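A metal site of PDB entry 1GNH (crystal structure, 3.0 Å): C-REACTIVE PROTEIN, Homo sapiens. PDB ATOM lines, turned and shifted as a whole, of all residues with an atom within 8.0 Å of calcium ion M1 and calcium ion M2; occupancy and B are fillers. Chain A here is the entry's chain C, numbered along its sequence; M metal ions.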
ATOM      1  N   SER A  50     -26.208 -16.331 -11.034  1.00  0.00           N
ATOM      2  CA  SER A  50     -25.574 -16.825 -12.239  1.00  0.00           C
ATOM      3  C   SER A  50     -25.035 -18.220 -12.047  1.00  0.00           C
ATOM      4  O   SER A  50     -24.312 -18.501 -11.097  1.00  0.00           O
ATOM      5  CB  SER A  50     -24.440 -15.898 -12.645  1.00  0.00           C
ATOM      6  OG  SER A  50     -23.749 -16.404 -13.781  1.00  0.00           O
ATOM      7  N   SER A  53     -21.394 -18.492 -16.834  1.00  0.00           N
ATOM      8  CA  SER A  53     -21.165 -17.247 -17.577  1.00  0.00           C
ATOM      9  C   SER A  53     -19.996 -17.324 -18.578  1.00  0.00           C
ATOM     10  O   SER A  53     -18.829 -17.311 -18.186  1.00  0.00           O
ATOM     11  CB  SER A  53     -20.922 -16.096 -16.610  1.00  0.00           C
ATOM     12  OG  SER A  53     -20.947 -14.835 -17.272  1.00  0.00           O
ATOM     13  N   ALA A  55     -18.233 -15.353 -21.429  1.00  0.00           N
ATOM     14  CA  ALA A  55     -18.111 -14.003 -21.995  1.00  0.00           C
ATOM     15  C   ALA A  55     -16.986 -13.791 -23.006  1.00  0.00           C
ATOM     16  O   ALA A  55     -15.922 -14.399 -22.916  1.00  0.00           O
ATOM     17  CB  ALA A  55     -17.972 -13.012 -20.864  1.00  0.00           C
ATOM     18  N   GLN A  59     -18.914  -9.409 -26.601  1.00  0.00           N
ATOM     19  CA  GLN A  59     -20.213  -9.690 -25.971  1.00  0.00           C
ATOM     20  C   GLN A  59     -19.991 -10.311 -24.589  1.00  0.00           C
ATOM     21  O   GLN A  59     -19.489 -11.428 -24.496  1.00  0.00           O
ATOM     22  CB  GLN A  59     -21.021 -10.630 -26.896  1.00  0.00           C
ATOM     23  CG  GLN A  59     -22.293 -11.189 -26.313  1.00  0.00           C
ATOM     24  CD  GLN A  59     -23.283 -10.121 -25.880  1.00  0.00           C
ATOM     25  OE1 GLN A  59     -23.200  -9.604 -24.772  1.00  0.00           O
ATOM     26  NE2 GLN A  59     -24.224  -9.817 -26.752  1.00  0.00           N
ATOM     27  N   ASP A  60     -20.372  -9.608 -23.541  1.00  0.00           N
ATOM     28  CA  ASP A  60     -20.198 -10.086 -22.179  1.00  0.00           C
ATOM     29  C   ASP A  60     -21.093 -11.274 -21.823  1.00  0.00           C
ATOM     30  O   ASP A  60     -20.777 -12.086 -20.940  1.00  0.00           O
ATOM     31  CB  ASP A  60     -20.410  -8.957 -21.157  1.00  0.00           C
ATOM     32  CG  ASP A  60     -21.814  -8.373 -21.205  1.00  0.00           C
ATOM     33  OD1 ASP A  60     -22.270  -7.983 -22.312  1.00  0.00           O
ATOM     34  OD2 ASP A  60     -22.463  -8.269 -20.150  1.00  0.00           O
ATOM     35  N   ASN A  61     -22.233 -11.390 -22.499  1.00  0.00           N
ATOM     36  CA  ASN A  61     -23.133 -12.498 -22.229  1.00  0.00           C
ATOM     37  C   ASN A  61     -23.278 -13.350 -23.471  1.00  0.00           C
ATOM     38  O   ASN A  61     -24.364 -13.443 -24.046  1.00  0.00           O
ATOM     39  CB  ASN A  61     -24.506 -11.976 -21.779  1.00  0.00           C
ATOM     40  CG  ASN A  61     -24.456 -11.290 -20.427  1.00  0.00           C
ATOM     41  OD1 ASN A  61     -23.579 -11.584 -19.630  1.00  0.00           O
ATOM     42  ND2 ASN A  61     -25.396 -10.379 -20.171  1.00  0.00           N
ATOM     43  N   GLU A  62     -22.175 -13.968 -23.905  1.00  0.00           N
ATOM     44  CA  GLU A  62     -22.147 -14.805 -25.103  1.00  0.00           C
ATOM     45  C   GLU A  62     -23.053 -16.026 -24.915  1.00  0.00           C
ATOM     46  O   GLU A  62     -23.777 -16.425 -25.814  1.00  0.00           O
ATOM     47  CB  GLU A  62     -20.724 -15.221 -25.443  1.00  0.00           C
ATOM     48  CG  GLU A  62     -20.548 -15.782 -26.850  1.00  0.00           C
ATOM     49  CD  GLU A  62     -20.795 -14.749 -27.943  1.00  0.00           C
ATOM     50  OE1 GLU A  62     -21.899 -14.149 -27.963  1.00  0.00           O
ATOM     51  OE2 GLU A  62     -19.892 -14.546 -28.795  1.00  0.00           O
ATOM     52  N   LEU A  64     -25.034 -17.625 -21.352  1.00  0.00           N
ATOM     53  CA  LEU A  64     -25.231 -17.496 -19.925  1.00  0.00           C
ATOM     54  C   LEU A  64     -26.483 -18.236 -19.419  1.00  0.00           C
ATOM     55  O   LEU A  64     -27.566 -18.125 -20.008  1.00  0.00           O
ATOM     56  CB  LEU A  64     -25.322 -16.021 -19.560  1.00  0.00           C
ATOM     57  CG  LEU A  64     -25.808 -15.628 -18.159  1.00  0.00           C
ATOM     58  CD1 LEU A  64     -24.705 -14.981 -17.366  1.00  0.00           C
ATOM     59  CD2 LEU A  64     -26.950 -14.682 -18.303  1.00  0.00           C
ATOM     60  N   PHE A  66     -28.857 -18.644 -16.166  1.00  0.00           N
ATOM     61  CA  PHE A  66     -29.193 -17.884 -14.976  1.00  0.00           C
ATOM     62  C   PHE A  66     -30.550 -18.297 -14.412  1.00  0.00           C
ATOM     63  O   PHE A  66     -31.438 -18.716 -15.164  1.00  0.00           O
ATOM     64  CB  PHE A  66     -29.247 -16.415 -15.416  1.00  0.00           C
ATOM     65  CG  PHE A  66     -29.338 -15.435 -14.294  1.00  0.00           C
ATOM     66  CD1 PHE A  66     -30.575 -15.026 -13.784  1.00  0.00           C
ATOM     67  CD2 PHE A  66     -28.180 -14.867 -13.781  1.00  0.00           C
ATOM     68  CE1 PHE A  66     -30.651 -14.059 -12.781  1.00  0.00           C
ATOM     69  CE2 PHE A  66     -28.246 -13.908 -12.772  1.00  0.00           C
ATOM     70  CZ  PHE A  66     -29.483 -13.498 -12.262  1.00  0.00           C
ATOM     71  N   GLN A 137     -20.001 -16.215 -10.504  1.00  0.00           N
ATOM     72  CA  GLN A 137     -20.175 -14.775 -10.608  1.00  0.00           C
ATOM     73  C   GLN A 137     -20.787 -14.431 -11.935  1.00  0.00           C
ATOM     74  O   GLN A 137     -20.687 -15.224 -12.893  1.00  0.00           O
ATOM     75  CB  GLN A 137     -18.848 -14.041 -10.475  1.00  0.00           C
ATOM     76  CG  GLN A 137     -18.395 -13.857  -9.045  1.00  0.00           C
ATOM     77  CD  GLN A 137     -19.445 -13.181  -8.161  1.00  0.00           C
ATOM     78  OE1 GLN A 137     -19.376 -13.294  -6.918  1.00  0.00           O
ATOM     79  NE2 GLN A 137     -20.407 -12.459  -8.775  1.00  0.00           N
ATOM     80  N   GLU A 138     -21.411 -13.251 -12.010  1.00  0.00           N
ATOM     81  CA  GLU A 138     -22.049 -12.819 -13.250  1.00  0.00           C
ATOM     82  C   GLU A 138     -21.170 -11.816 -13.984  1.00  0.00           C
ATOM     83  O   GLU A 138     -20.989 -10.688 -13.508  1.00  0.00           O
ATOM     84  CB  GLU A 138     -23.420 -12.206 -12.964  1.00  0.00           C
ATOM     85  CG  GLU A 138     -24.387 -12.283 -14.132  1.00  0.00           C
ATOM     86  CD  GLU A 138     -24.026 -11.380 -15.313  1.00  0.00           C
ATOM     87  OE1 GLU A 138     -24.438 -10.192 -15.308  1.00  0.00           O
ATOM     88  OE2 GLU A 138     -23.383 -11.881 -16.268  1.00  0.00           O
ATOM     89  N   GLN A 139     -20.619 -12.225 -15.125  1.00  0.00           N
ATOM     90  CA  GLN A 139     -19.759 -11.345 -15.914  1.00  0.00           C
ATOM     91  C   GLN A 139     -20.532 -10.261 -16.681  1.00  0.00           C
ATOM     92  O   GLN A 139     -21.559 -10.508 -17.333  1.00  0.00           O
ATOM     93  CB  GLN A 139     -18.943 -12.149 -16.911  1.00  0.00           C
ATOM     94  CG  GLN A 139     -17.576 -12.500 -16.437  1.00  0.00           C
ATOM     95  CD  GLN A 139     -16.993 -13.666 -17.226  1.00  0.00           C
ATOM     96  OE1 GLN A 139     -17.172 -14.817 -16.851  1.00  0.00           O
ATOM     97  NE2 GLN A 139     -16.343 -13.367 -18.336  1.00  0.00           N
ATOM     98  N   ASP A 140     -19.998  -9.040 -16.601  1.00  0.00           N
ATOM     99  CA  ASP A 140     -20.578  -7.900 -17.277  1.00  0.00           C
ATOM    100  C   ASP A 140     -19.469  -7.189 -18.054  1.00  0.00           C
ATOM    101  O   ASP A 140     -19.649  -6.092 -18.583  1.00  0.00           O
ATOM    102  CB  ASP A 140     -21.278  -6.991 -16.261  1.00  0.00           C
ATOM    103  CG  ASP A 140     -22.591  -7.591 -15.771  1.00  0.00           C
ATOM    104  OD1 ASP A 140     -23.319  -8.185 -16.598  1.00  0.00           O
ATOM    105  OD2 ASP A 140     -22.896  -7.477 -14.558  1.00  0.00           O
ATOM    106  N   SER A 141     -18.317  -7.852 -18.109  1.00  0.00           N
ATOM    107  CA  SER A 141     -17.150  -7.379 -18.821  1.00  0.00           C
ATOM    108  C   SER A 141     -16.227  -8.575 -18.883  1.00  0.00           C
ATOM    109  O   SER A 141     -16.276  -9.432 -18.007  1.00  0.00           O
ATOM    110  CB  SER A 141     -16.463  -6.210 -18.091  1.00  0.00           C
ATOM    111  OG  SER A 141     -15.625  -6.631 -17.034  1.00  0.00           O
ATOM    112  N   GLY A 144     -14.690  -9.724 -15.634  1.00  0.00           N
ATOM    113  CA  GLY A 144     -14.953  -8.884 -14.483  1.00  0.00           C
ATOM    114  C   GLY A 144     -16.322  -8.227 -14.419  1.00  0.00           C
ATOM    115  O   GLY A 144     -17.244  -8.626 -15.122  1.00  0.00           O
ATOM    116  N   ASN A 145     -16.415  -7.193 -13.579  1.00  0.00           N
ATOM    117  CA  ASN A 145     -17.634  -6.418 -13.357  1.00  0.00           C
ATOM    118  C   ASN A 145     -18.692  -7.303 -12.733  1.00  0.00           C
ATOM    119  O   ASN A 145     -19.794  -7.454 -13.258  1.00  0.00           O
ATOM    120  CB  ASN A 145     -18.132  -5.785 -14.659  1.00  0.00           C
ATOM    121  CG  ASN A 145     -17.396  -4.480 -14.997  1.00  0.00           C
ATOM    122  OD1 ASN A 145     -16.181  -4.468 -15.228  1.00  0.00           O
ATOM    123  ND2 ASN A 145     -18.142  -3.390 -15.049  1.00  0.00           N
ATOM    124  N   PHE A 146     -18.363  -7.841 -11.569  1.00  0.00           N
ATOM    125  CA  PHE A 146     -19.236  -8.752 -10.845  1.00  0.00           C
ATOM    126  C   PHE A 146     -20.249  -8.087  -9.939  1.00  0.00           C
ATOM    127  O   PHE A 146     -19.882  -7.304  -9.064  1.00  0.00           O
ATOM    128  CB  PHE A 146     -18.396  -9.724 -10.018  1.00  0.00           C
ATOM    129  CG  PHE A 146     -17.370 -10.496 -10.820  1.00  0.00           C
ATOM    130  CD1 PHE A 146     -17.658 -10.979 -12.098  1.00  0.00           C
ATOM    131  CD2 PHE A 146     -16.097 -10.725 -10.300  1.00  0.00           C
ATOM    132  CE1 PHE A 146     -16.697 -11.671 -12.824  1.00  0.00           C
ATOM    133  CE2 PHE A 146     -15.139 -11.419 -11.040  1.00  0.00           C
ATOM    134  CZ  PHE A 146     -15.446 -11.882 -12.295  1.00  0.00           C
ATOM    135  N   GLU A 147     -21.519  -8.398 -10.129  1.00  0.00           N
ATOM    136  CA  GLU A 147     -22.567  -7.868  -9.265  1.00  0.00           C
ATOM    137  C   GLU A 147     -22.845  -8.928  -8.217  1.00  0.00           C
ATOM    138  O   GLU A 147     -23.231 -10.053  -8.549  1.00  0.00           O
ATOM    139  CB  GLU A 147     -23.832  -7.592 -10.060  1.00  0.00           C
ATOM    140  CG  GLU A 147     -23.669  -6.481 -11.038  1.00  0.00           C
ATOM    141  CD  GLU A 147     -24.877  -6.316 -11.901  1.00  0.00           C
ATOM    142  OE1 GLU A 147     -25.072  -7.212 -12.776  1.00  0.00           O
ATOM    143  OE2 GLU A 147     -25.603  -5.314 -11.706  1.00  0.00           O
ATOM    144  N   GLY A 148     -22.632  -8.573  -6.958  1.00  0.00           N
ATOM    145  CA  GLY A 148     -22.855  -9.504  -5.857  1.00  0.00           C
ATOM    146  C   GLY A 148     -24.278  -9.991  -5.692  1.00  0.00           C
ATOM    147  O   GLY A 148     -24.520 -11.000  -5.009  1.00  0.00           O
ATOM    148  N   SER A 149     -25.216  -9.296  -6.315  1.00  0.00           N
ATOM    149  CA  SER A 149     -26.631  -9.643  -6.265  1.00  0.00           C
ATOM    150  C   SER A 149     -26.928 -10.803  -7.217  1.00  0.00           C
ATOM    151  O   SER A 149     -28.059 -11.282  -7.310  1.00  0.00           O
ATOM    152  CB  SER A 149     -27.460  -8.408  -6.661  1.00  0.00           C
ATOM    153  OG  SER A 149     -28.855  -8.613  -6.486  1.00  0.00           O
ATOM    154  N   GLN A 150     -25.896 -11.244  -7.931  1.00  0.00           N
ATOM    155  CA  GLN A 150     -26.034 -12.324  -8.884  1.00  0.00           C
ATOM    156  C   GLN A 150     -24.972 -13.386  -8.656  1.00  0.00           C
ATOM    157  O   GLN A 150     -24.650 -14.162  -9.552  1.00  0.00           O
ATOM    158  CB  GLN A 150     -25.938 -11.764 -10.295  1.00  0.00           C
ATOM    159  CG  GLN A 150     -26.798 -10.520 -10.500  1.00  0.00           C
ATOM    160  CD  GLN A 150     -26.898 -10.093 -11.967  1.00  0.00           C
ATOM    161  OE1 GLN A 150     -25.893  -9.837 -12.632  1.00  0.00           O
ATOM    162  NE2 GLN A 150     -28.129  -9.996 -12.459  1.00  0.00           N
HETATM  163 CA    CA M   1     -23.795  -9.840 -17.576  1.00  0.00          CA
HETATM  164 CA    CA M   2     -24.404  -8.652 -13.974  1.00  0.00          CA
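The nearest printed residue that does not touch calcium ion M2 is Gln 139 (4.8 Å).
Residues that only touch calcium ion M1: Asp 60 (3.3 Å). Of the 21 residues printed, 5 come within 4 Å of calcium ion M1. The nearest printed residue that does not touch calcium ion M1 is Leu 64 (5.2 Å).
Calcium ion M1 is bound by the side-chain carboxylate (OD1) of Asp 140, at 2.0 Å. O of Gln 139 is bound to calcium ion M1, 2.3 Å away. The side-chain carboxylate (OE1) of Glu 138 binds calcium ion M1. The side-chain carboxylate (OE2) of Glu 138 binds calcium ion M1, at 2.5 Å. Calcium ion M1 is bound by OD1 of Asn 61 (2.7 Å). Slightly farther from calcium ion M1 lies the side-chain amide nitrogen (ND2) of Asn 61 (3.1 Å).
Calcium ion M2 is bound by OE1 of Glu 147 (2.0 Å), OD2 of Asp 140 (2.0 Å), OE1 of Glu 138 (2.0 Å), OE1 of Gln 150 (2.3 Å) and OD1 of Asp 140 (2.9 Å).
O of Gln 150 lies within hydrogen-bond range of N of Ser 50, at 3.1 Å. OE1 of Gln 139 lies close to O of Ser 53 (3.3 Å). The backbone NH of Asn 61 sits at hydrogen-bond distance from the side-chain amide oxygen of Gln 59, at 3.0 Å. The side-chain carboxylate of Asp 60 lies close to the side-chain amide oxygen of Gln 59 (3.1 Å).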
